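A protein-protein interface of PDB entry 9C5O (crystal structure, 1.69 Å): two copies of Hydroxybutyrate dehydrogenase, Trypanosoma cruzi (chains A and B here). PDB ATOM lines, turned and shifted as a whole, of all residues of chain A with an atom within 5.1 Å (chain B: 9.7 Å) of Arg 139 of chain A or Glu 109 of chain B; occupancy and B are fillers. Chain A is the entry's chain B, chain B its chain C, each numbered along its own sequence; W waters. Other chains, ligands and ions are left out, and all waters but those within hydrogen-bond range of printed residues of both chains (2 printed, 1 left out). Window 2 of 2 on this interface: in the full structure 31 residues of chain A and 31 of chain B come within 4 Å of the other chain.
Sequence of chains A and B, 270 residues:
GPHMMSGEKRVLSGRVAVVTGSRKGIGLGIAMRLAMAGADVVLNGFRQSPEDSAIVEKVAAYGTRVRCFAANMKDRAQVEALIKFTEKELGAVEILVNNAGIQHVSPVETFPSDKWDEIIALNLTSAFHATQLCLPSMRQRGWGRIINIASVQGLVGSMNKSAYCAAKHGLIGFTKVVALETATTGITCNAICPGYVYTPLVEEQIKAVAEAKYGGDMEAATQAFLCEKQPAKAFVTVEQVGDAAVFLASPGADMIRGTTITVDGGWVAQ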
ATOM      1  N   GLN A 132     -18.190  -4.087   1.624  1.00  0.00           N
ATOM      2  CA  GLN A 132     -18.258  -2.794   2.295  1.00  0.00           C
ATOM      3  C   GLN A 132     -19.271  -2.831   3.429  1.00  0.00           C
ATOM      4  O   GLN A 132     -19.058  -2.237   4.504  1.00  0.00           O
ATOM      5  CB  GLN A 132     -18.624  -1.732   1.242  1.00  0.00           C
ATOM      6  CG  GLN A 132     -18.549  -0.356   1.688  1.00  0.00           C
ATOM      7  CD  GLN A 132     -18.759   0.624   0.525  1.00  0.00           C
ATOM      8  OE1 GLN A 132     -19.817   0.632  -0.103  1.00  0.00           O
ATOM      9  NE2 GLN A 132     -17.732   1.395   0.200  1.00  0.00           N
ATOM     10  N   LEU A 135     -17.812  -5.301   6.475  1.00  0.00           N
ATOM     11  CA  LEU A 135     -16.552  -5.047   7.172  1.00  0.00           C
ATOM     12  C   LEU A 135     -16.682  -4.327   8.502  1.00  0.00           C
ATOM     13  O   LEU A 135     -15.929  -4.677   9.428  1.00  0.00           O
ATOM     14  CB  LEU A 135     -15.610  -4.278   6.243  1.00  0.00           C
ATOM     15  CG  LEU A 135     -14.786  -5.104   5.271  1.00  0.00           C
ATOM     16  CD1 LEU A 135     -14.134  -4.169   4.235  1.00  0.00           C
ATOM     17  CD2 LEU A 135     -13.707  -5.911   5.974  1.00  0.00           C
ATOM     18  N   PRO A 136     -17.507  -3.287   8.660  1.00  0.00           N
ATOM     19  CA  PRO A 136     -17.528  -2.585   9.956  1.00  0.00           C
ATOM     20  C   PRO A 136     -17.826  -3.502  11.136  1.00  0.00           C
ATOM     21  O   PRO A 136     -17.182  -3.385  12.182  1.00  0.00           O
ATOM     22  CB  PRO A 136     -18.614  -1.518   9.749  1.00  0.00           C
ATOM     23  CG  PRO A 136     -18.546  -1.236   8.221  1.00  0.00           C
ATOM     24  CD  PRO A 136     -18.356  -2.628   7.643  1.00  0.00           C
ATOM     25  N   SER A 137     -18.783  -4.426  10.996  1.00  0.00           N
ATOM     26  CA  SER A 137     -19.083  -5.336  12.097  1.00  0.00           C
ATOM     27  C   SER A 137     -17.917  -6.293  12.365  1.00  0.00           C
ATOM     28  O   SER A 137     -17.572  -6.568  13.516  1.00  0.00           O
ATOM     29  CB  SER A 137     -20.350  -6.133  11.773  1.00  0.00           C
ATOM     30  OG  SER A 137     -20.599  -7.124  12.759  1.00  0.00           O
ATOM     31  N   MET A 138     -17.347  -6.864  11.306  1.00  0.00           N
ATOM     32  CA  MET A 138     -16.150  -7.682  11.426  1.00  0.00           C
ATOM     33  C   MET A 138     -15.028  -6.977  12.180  1.00  0.00           C
ATOM     34  O   MET A 138     -14.384  -7.560  13.061  1.00  0.00           O
ATOM     35  CB  MET A 138     -15.772  -8.036  10.002  1.00  0.00           C
ATOM     36  CG  MET A 138     -16.723  -9.033   9.325  1.00  0.00           C
ATOM     37  SD  MET A 138     -16.082  -9.492   7.714  1.00  0.00           S
ATOM     38  CE  MET A 138     -17.438 -10.537   7.136  1.00  0.00           C
ATOM     39  N   ARG A 139     -14.775  -5.721  11.835  1.00  0.00           N
ATOM     40  CA  ARG A 139     -13.734  -4.983  12.528  1.00  0.00           C
ATOM     41  C   ARG A 139     -14.096  -4.801  13.997  1.00  0.00           C
ATOM     42  O   ARG A 139     -13.241  -4.962  14.878  1.00  0.00           O
ATOM     43  CB  ARG A 139     -13.503  -3.624  11.858  1.00  0.00           C
ATOM     44  CG  ARG A 139     -12.810  -3.702  10.508  1.00  0.00           C
ATOM     45  CD  ARG A 139     -12.432  -2.290  10.010  1.00  0.00           C
ATOM     46  NE  ARG A 139     -11.649  -2.296   8.775  1.00  0.00           N
ATOM     47  CZ  ARG A 139     -10.332  -2.462   8.745  1.00  0.00           C
ATOM     48  NH1 ARG A 139      -9.660  -2.808   9.830  1.00  0.00           N
ATOM     49  NH2 ARG A 139      -9.673  -2.247   7.608  1.00  0.00           N
ATOM     50  N   GLN A 140     -15.373  -4.496  14.280  1.00  0.00           N
ATOM     51  CA  GLN A 140     -15.808  -4.295  15.664  1.00  0.00           C
ATOM     52  C   GLN A 140     -15.593  -5.551  16.502  1.00  0.00           C
ATOM     53  O   GLN A 140     -15.181  -5.470  17.664  1.00  0.00           O
ATOM     54  CB  GLN A 140     -17.283  -3.874  15.695  1.00  0.00           C
ATOM     55  CG  GLN A 140     -17.653  -2.490  15.107  1.00  0.00           C
ATOM     56  CD  GLN A 140     -19.149  -2.204  15.123  1.00  0.00           C
ATOM     57  OE1 GLN A 140     -19.968  -3.128  15.125  1.00  0.00           O
ATOM     58  NE2 GLN A 140     -19.509  -0.922  15.092  1.00  0.00           N
ATOM     59  N   ARG A 141     -15.890  -6.716  15.932  1.00  0.00           N
ATOM     60  CA  ARG A 141     -15.733  -8.001  16.610  1.00  0.00           C
ATOM     61  C   ARG A 141     -14.349  -8.571  16.573  1.00  0.00           C
ATOM     62  O   ARG A 141     -14.042  -9.407  17.424  1.00  0.00           O
ATOM     63  CB  ARG A 141     -16.698  -9.011  16.022  1.00  0.00           C
ATOM     64  CG  ARG A 141     -17.980  -8.431  15.977  1.00  0.00           C
ATOM     65  CD  ARG A 141     -18.941  -8.978  17.123  1.00  0.00           C
ATOM     66  NE  ARG A 141     -19.808 -10.037  16.571  1.00  0.00           N
ATOM     67  CZ  ARG A 141     -19.988 -11.223  17.138  1.00  0.00           C
ATOM     68  NH1 ARG A 141     -19.516 -11.459  18.336  1.00  0.00           N
ATOM     69  NH2 ARG A 141     -20.726 -12.165  16.523  1.00  0.00           N
ATOM     70  N   GLY A 142     -13.512  -8.119  15.651  1.00  0.00           N
ATOM     71  CA  GLY A 142     -12.147  -8.590  15.564  1.00  0.00           C
ATOM     72  C   GLY A 142     -11.984  -9.898  14.834  1.00  0.00           C
ATOM     73  O   GLY A 142     -10.976 -10.594  15.030  1.00  0.00           O
ATOM     74  N   GLU A 181      -5.832  -4.130   3.567  1.00  0.00           N
ATOM     75  CA  GLU A 181      -6.431  -3.176   4.488  1.00  0.00           C
ATOM     76  C   GLU A 181      -6.789  -3.799   5.827  1.00  0.00           C
ATOM     77  O   GLU A 181      -6.921  -3.062   6.804  1.00  0.00           O
ATOM     78  CB  GLU A 181      -7.678  -2.529   3.879  1.00  0.00           C
ATOM     79  CG  GLU A 181      -7.329  -1.661   2.675  1.00  0.00           C
ATOM     80  CD  GLU A 181      -8.515  -0.886   2.102  1.00  0.00           C
ATOM     81  OE1 GLU A 181      -9.589  -0.817   2.762  1.00  0.00           O
ATOM     82  OE2 GLU A 181      -8.358  -0.327   0.996  1.00  0.00           O
ATOM     83  N   THR A 182      -6.935  -5.122   5.892  1.00  0.00           N
ATOM     84  CA  THR A 182      -7.302  -5.815   7.117  1.00  0.00           C
ATOM     85  C   THR A 182      -6.168  -6.676   7.675  1.00  0.00           C
ATOM     86  O   THR A 182      -6.395  -7.469   8.594  1.00  0.00           O
ATOM     87  CB  THR A 182      -8.533  -6.699   6.874  1.00  0.00           C
ATOM     88  OG1 THR A 182      -8.285  -7.645   5.815  1.00  0.00           O
ATOM     89  CG2 THR A 182      -9.769  -5.886   6.503  1.00  0.00           C
ATOM     90  N   THR A 185      -5.547  -7.428  11.426  1.00  0.00           N
ATOM     91  CA  THR A 185      -6.742  -7.788  12.173  1.00  0.00           C
ATOM     92  C   THR A 185      -6.977  -9.282  12.053  1.00  0.00           C
ATOM     93  O   THR A 185      -6.314  -9.954  11.281  1.00  0.00           O
ATOM     94  CB  THR A 185      -7.979  -7.052  11.653  1.00  0.00           C
ATOM     95  OG1 THR A 185      -8.411  -7.608  10.405  1.00  0.00           O
ATOM     96  CG2 THR A 185      -7.719  -5.524  11.462  1.00  0.00           C
ATOM     97  N   ILE A 187      -9.448 -10.392  10.473  1.00  0.00           N
ATOM     98  CA  ILE A 187     -10.218 -10.515   9.245  1.00  0.00           C
ATOM     99  C   ILE A 187      -9.255 -10.893   8.131  1.00  0.00           C
ATOM    100  O   ILE A 187      -8.242 -10.216   7.932  1.00  0.00           O
ATOM    101  CB  ILE A 187     -10.938  -9.205   8.901  1.00  0.00           C
ATOM    102  CG1 ILE A 187     -11.854  -8.754  10.047  1.00  0.00           C
ATOM    103  CG2 ILE A 187     -11.676  -9.342   7.563  1.00  0.00           C
ATOM    104  CD1 ILE A 187     -12.182  -7.281   9.924  1.00  0.00           C
ATOM    105  N   VAL B 105      -8.467   7.562  -3.801  1.00  0.00           N
ATOM    106  CA  VAL B 105      -7.892   6.851  -2.657  1.00  0.00           C
ATOM    107  C   VAL B 105      -8.845   6.927  -1.467  1.00  0.00           C
ATOM    108  O   VAL B 105      -9.176   8.016  -0.979  1.00  0.00           O
ATOM    109  CB  VAL B 105      -6.511   7.430  -2.294  1.00  0.00           C
ATOM    110  CG1 VAL B 105      -5.901   6.712  -1.092  1.00  0.00           C
ATOM    111  CG2 VAL B 105      -5.569   7.383  -3.510  1.00  0.00           C
ATOM    112  N   SER B 106      -9.221   5.772  -0.955  1.00  0.00           N
ATOM    113  CA  SER B 106     -10.136   5.636   0.162  1.00  0.00           C
ATOM    114  C   SER B 106     -10.087   4.218   0.700  1.00  0.00           C
ATOM    115  O   SER B 106      -9.980   3.272  -0.089  1.00  0.00           O
ATOM    116  CB  SER B 106     -11.569   5.946  -0.261  1.00  0.00           C
ATOM    117  OG  SER B 106     -12.461   5.608   0.780  1.00  0.00           O
ATOM    118  N   PRO B 107     -10.223   4.011   2.004  1.00  0.00           N
ATOM    119  CA  PRO B 107     -10.453   2.636   2.486  1.00  0.00           C
ATOM    120  C   PRO B 107     -11.737   2.093   1.870  1.00  0.00           C
ATOM    121  O   PRO B 107     -12.624   2.847   1.459  1.00  0.00           O
ATOM    122  CB  PRO B 107     -10.582   2.786   4.006  1.00  0.00           C
ATOM    123  CG  PRO B 107      -9.993   4.180   4.312  1.00  0.00           C
ATOM    124  CD  PRO B 107     -10.236   5.013   3.088  1.00  0.00           C
ATOM    125  N   VAL B 108     -11.834   0.764   1.826  1.00  0.00           N
ATOM    126  CA  VAL B 108     -12.989   0.105   1.217  1.00  0.00           C
ATOM    127  C   VAL B 108     -14.293   0.508   1.901  1.00  0.00           C
ATOM    128  O   VAL B 108     -15.317   0.706   1.229  1.00  0.00           O
ATOM    129  CB  VAL B 108     -12.796  -1.421   1.250  1.00  0.00           C
ATOM    130  CG1 VAL B 108     -14.093  -2.104   0.872  1.00  0.00           C
ATOM    131  CG2 VAL B 108     -11.694  -1.820   0.282  1.00  0.00           C
ATOM    132  N   GLU B 109     -14.284   0.631   3.231  1.00  0.00           N
ATOM    133  CA  GLU B 109     -15.534   0.826   3.974  1.00  0.00           C
ATOM    134  C   GLU B 109     -16.236   2.117   3.591  1.00  0.00           C
ATOM    135  O   GLU B 109     -17.468   2.199   3.645  1.00  0.00           O
ATOM    136  CB  GLU B 109     -15.282   0.834   5.483  1.00  0.00           C
ATOM    137  CG  GLU B 109     -14.875  -0.528   6.016  1.00  0.00           C
ATOM    138  CD  GLU B 109     -13.372  -0.748   6.016  1.00  0.00           C
ATOM    139  OE1 GLU B 109     -12.635  -0.001   5.329  1.00  0.00           O
ATOM    140  OE2 GLU B 109     -12.928  -1.688   6.715  1.00  0.00           O
ATOM    141  N   THR B 110     -15.469   3.145   3.256  1.00  0.00           N
ATOM    142  CA  THR B 110     -16.012   4.453   2.934  1.00  0.00           C
ATOM    143  C   THR B 110     -15.838   4.808   1.462  1.00  0.00           C
ATOM    144  O   THR B 110     -16.091   5.956   1.082  1.00  0.00           O
ATOM    145  CB  THR B 110     -15.349   5.514   3.815  1.00  0.00           C
ATOM    146  OG1 THR B 110     -13.931   5.436   3.625  1.00  0.00           O
ATOM    147  CG2 THR B 110     -15.695   5.300   5.281  1.00  0.00           C
ATOM    148  N   PHE B 111     -15.467   3.852   0.617  1.00  0.00           N
ATOM    149  CA  PHE B 111     -15.238   4.133  -0.793  1.00  0.00           C
ATOM    150  C   PHE B 111     -16.554   4.535  -1.458  1.00  0.00           C
ATOM    151  O   PHE B 111     -17.500   3.749  -1.438  1.00  0.00           O
ATOM    152  CB  PHE B 111     -14.637   2.902  -1.482  1.00  0.00           C
ATOM    153  CG  PHE B 111     -13.792   3.251  -2.658  1.00  0.00           C
ATOM    154  CD1 PHE B 111     -14.375   3.719  -3.841  1.00  0.00           C
ATOM    155  CD2 PHE B 111     -12.406   3.160  -2.578  1.00  0.00           C
ATOM    156  CE1 PHE B 111     -13.590   4.095  -4.935  1.00  0.00           C
ATOM    157  CE2 PHE B 111     -11.609   3.517  -3.674  1.00  0.00           C
ATOM    158  CZ  PHE B 111     -12.207   4.005  -4.862  1.00  0.00           C
ATOM    159  N   PRO B 112     -16.681   5.746  -2.016  1.00  0.00           N
ATOM    160  CA  PRO B 112     -17.988   6.166  -2.549  1.00  0.00           C
ATOM    161  C   PRO B 112     -18.398   5.291  -3.724  1.00  0.00           C
ATOM    162  O   PRO B 112     -17.592   4.988  -4.600  1.00  0.00           O
ATOM    163  CB  PRO B 112     -17.750   7.619  -2.980  1.00  0.00           C
ATOM    164  CG  PRO B 112     -16.545   8.073  -2.194  1.00  0.00           C
ATOM    165  CD  PRO B 112     -15.684   6.830  -2.061  1.00  0.00           C
ATOM    166  N   SER B 113     -19.678   4.908  -3.747  1.00  0.00           N
ATOM    167  CA  SER B 113     -20.155   4.034  -4.809  1.00  0.00           C
ATOM    168  C   SER B 113     -19.950   4.666  -6.177  1.00  0.00           C
ATOM    169  O   SER B 113     -19.587   3.972  -7.126  1.00  0.00           O
ATOM    170  CB  SER B 113     -21.632   3.704  -4.598  1.00  0.00           C
ATOM    171  OG  SER B 113     -21.790   2.717  -3.604  1.00  0.00           O
ATOM    172  N   TRP B 116     -16.307   4.348  -7.295  1.00  0.00           N
ATOM    173  CA  TRP B 116     -16.068   2.975  -7.719  1.00  0.00           C
ATOM    174  C   TRP B 116     -16.594   2.776  -9.132  1.00  0.00           C
ATOM    175  O   TRP B 116     -15.856   2.350 -10.031  1.00  0.00           O
ATOM    176  CB  TRP B 116     -16.741   2.010  -6.728  1.00  0.00           C
ATOM    177  CG  TRP B 116     -16.659   0.590  -7.189  1.00  0.00           C
ATOM    178  CD1 TRP B 116     -17.437   0.013  -8.123  1.00  0.00           C
ATOM    179  CD2 TRP B 116     -15.711  -0.417  -6.776  1.00  0.00           C
ATOM    180  NE1 TRP B 116     -17.064  -1.290  -8.321  1.00  0.00           N
ATOM    181  CE2 TRP B 116     -16.009  -1.577  -7.499  1.00  0.00           C
ATOM    182  CE3 TRP B 116     -14.669  -0.455  -5.843  1.00  0.00           C
ATOM    183  CZ2 TRP B 116     -15.292  -2.761  -7.351  1.00  0.00           C
ATOM    184  CZ3 TRP B 116     -13.956  -1.657  -5.679  1.00  0.00           C
ATOM    185  CH2 TRP B 116     -14.276  -2.783  -6.441  1.00  0.00           C
ATOM    186  N   MET B 159      -3.133  -0.827  -0.385  1.00  0.00           N
ATOM    187  CA  MET B 159      -4.167  -0.315   0.496  1.00  0.00           C
ATOM    188  C   MET B 159      -4.820   0.924  -0.099  1.00  0.00           C
ATOM    189  O   MET B 159      -4.140   1.792  -0.658  1.00  0.00           O
ATOM    190  CB  MET B 159      -3.571   0.026   1.874  1.00  0.00           C
ATOM    191  CG  MET B 159      -3.210  -1.233   2.698  1.00  0.00           C
ATOM    192  SD  MET B 159      -2.734  -0.873   4.379  1.00  0.00           S
ATOM    193  CE  MET B 159      -1.327   0.185   4.106  1.00  0.00           C
ATOM    194  N   ASN B 160      -6.136   1.025   0.095  1.00  0.00           N
ATOM    195  CA  ASN B 160      -6.916   2.226  -0.185  1.00  0.00           C
ATOM    196  C   ASN B 160      -7.108   2.452  -1.675  1.00  0.00           C
ATOM    197  O   ASN B 160      -7.557   3.539  -2.081  1.00  0.00           O
ATOM    198  CB  ASN B 160      -6.278   3.452   0.489  1.00  0.00           C
ATOM    199  CG  ASN B 160      -6.229   3.307   2.016  1.00  0.00           C
ATOM    200  OD1 ASN B 160      -7.138   2.726   2.622  1.00  0.00           O
ATOM    201  ND2 ASN B 160      -5.143   3.770   2.627  1.00  0.00           N
ATOM    202  N   LYS B 161      -6.830   1.452  -2.499  1.00  0.00           N
ATOM    203  CA  LYS B 161      -6.968   1.584  -3.932  1.00  0.00           C
ATOM    204  C   LYS B 161      -7.782   0.427  -4.471  1.00  0.00           C
ATOM    205  O   LYS B 161      -7.559  -0.050  -5.576  1.00  0.00           O
ATOM    206  CB  LYS B 161      -5.600   1.689  -4.597  1.00  0.00           C
ATOM    207  CG  LYS B 161      -4.895   3.041  -4.307  1.00  0.00           C
ATOM    208  CD  LYS B 161      -3.512   3.106  -4.922  1.00  0.00           C
ATOM    209  CE  LYS B 161      -2.852   4.446  -4.542  1.00  0.00           C
ATOM    210  NZ  LYS B 161      -1.540   4.673  -5.215  1.00  0.00           N
ATOM    211  N   SER B 162      -8.853   0.090  -3.768  1.00  0.00           N
ATOM    212  CA  SER B 162      -9.648  -1.072  -4.158  1.00  0.00           C
ATOM    213  C   SER B 162     -10.232  -0.951  -5.567  1.00  0.00           C
ATOM    214  O   SER B 162     -10.122  -1.885  -6.373  1.00  0.00           O
ATOM    215  CB  SER B 162     -10.739  -1.319  -3.115  1.00  0.00           C
ATOM    216  OG  SER B 162     -11.657  -0.262  -2.953  1.00  0.00           O
HETATM  217  O   HOH W   1     -19.507   0.388   5.084  1.00  0.00           O
HETATM  218  O   HOH W   2      -9.779   0.806  -1.069  1.00  0.00           O
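The backbone carbonyl oxygen of Val 108 of chain B is in hydrogen-bond range of the side-chain amide nitrogen of Gln 132 of chain A (2.7 Å).
The backbone carbonyl oxygen (O) of Phe 111 of chain B sits at hydrogen-bond distance from the side-chain amide nitrogen (NE2) of Gln 132 of chain A.
The guanidinium group (NE) of Arg 139 of chain A is in salt-bridge range of the side-chain carboxylate (OE2) of Glu 109 of chain B (2.5 Å).
The side-chain carboxylate of Glu 181 of chain A lies within hydrogen-bond range of the backbone NH of Val 108 of chain B, 2.9 Å away.
The backbone NH of Asn 160 of chain B lies within hydrogen-bond range of the side-chain carboxylate of Glu 181 of chain A, at 2.8 Å.
The guanidinium group (NH2) of Arg 139 of chain A lies within hydrogen-bond range of the backbone carbonyl oxygen (O) of Glu 181 of chain A, at 3.0 Å.
OG of Ser 106 of chain B is in hydrogen-bond range of N of Phe 111 of chain B (3.5 Å).
N of Ser 106 of chain B lies within hydrogen-bond range of O of Asn 160 of chain B (3.0 Å).
CG of Gln 132 of chain A touches O of Glu 109 of chain B (3.4 Å).
Leu 135 of chain A touches Val 108 of chain B.
Leu 135 of chain A touches Glu 109 of chain B.
Glu 181 of chain A touches Pro 107 of chain B.
C of Met 159 of chain B touches OE2 of Glu 181 of chain A, at 3.9 Å.
Leu 135 of chain A touches just these residues of chain B: Val 108 and Glu 109.
No residue of chain B comes within 4 Å of Pro 136 of chain A.
Arg 139 of chain A touches just one residue of chain B: Glu 109 (2.5 Å).
Of the printed residues of chain B, Glu 181 of chain A touches Pro 107 (3.6 Å), Val 108 (2.9 Å), Met 159 (3.9 Å) and Asn 160 (2.8 Å).
Val 105 of chain B touches none of the printed residues of chain A.
Of the printed residues of chain A, Pro 107 of chain B touches Glu 181.
Glu 109 of chain B touches three residues of chain A.
Of the printed residues of chain A, Phe 111 of chain B touches Gln 132.
Ser 113 of chain B touches none of the printed residues of chain A.
The nearest printed residue of chain A that does not touch Asn 160 of chain B is Arg 139 of chain A (7.5 Å).
Hydrophobic or aromatic side chains of chain A within 4 Å of the printed part of chain B: Leu 135.
No position is printed for both chains.
Of the 10 pairs that touch across the chains among the printed residues, none has its exchanged pair printed and touching as well.
Water W2 lies within hydrogen-bond range of O of Ser 106 of chain B (2.7 Å), OE2 of Glu 181 of chain A (2.8 Å), OG of Ser 162 of chain B (2.9 Å) and N of Lys 161 of chain B (3.3 Å).
Water W1 lies within hydrogen-bond range of O of Gln 132 of chain A (2.7 Å) and O of Glu 109 of chain B (3.1 Å).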
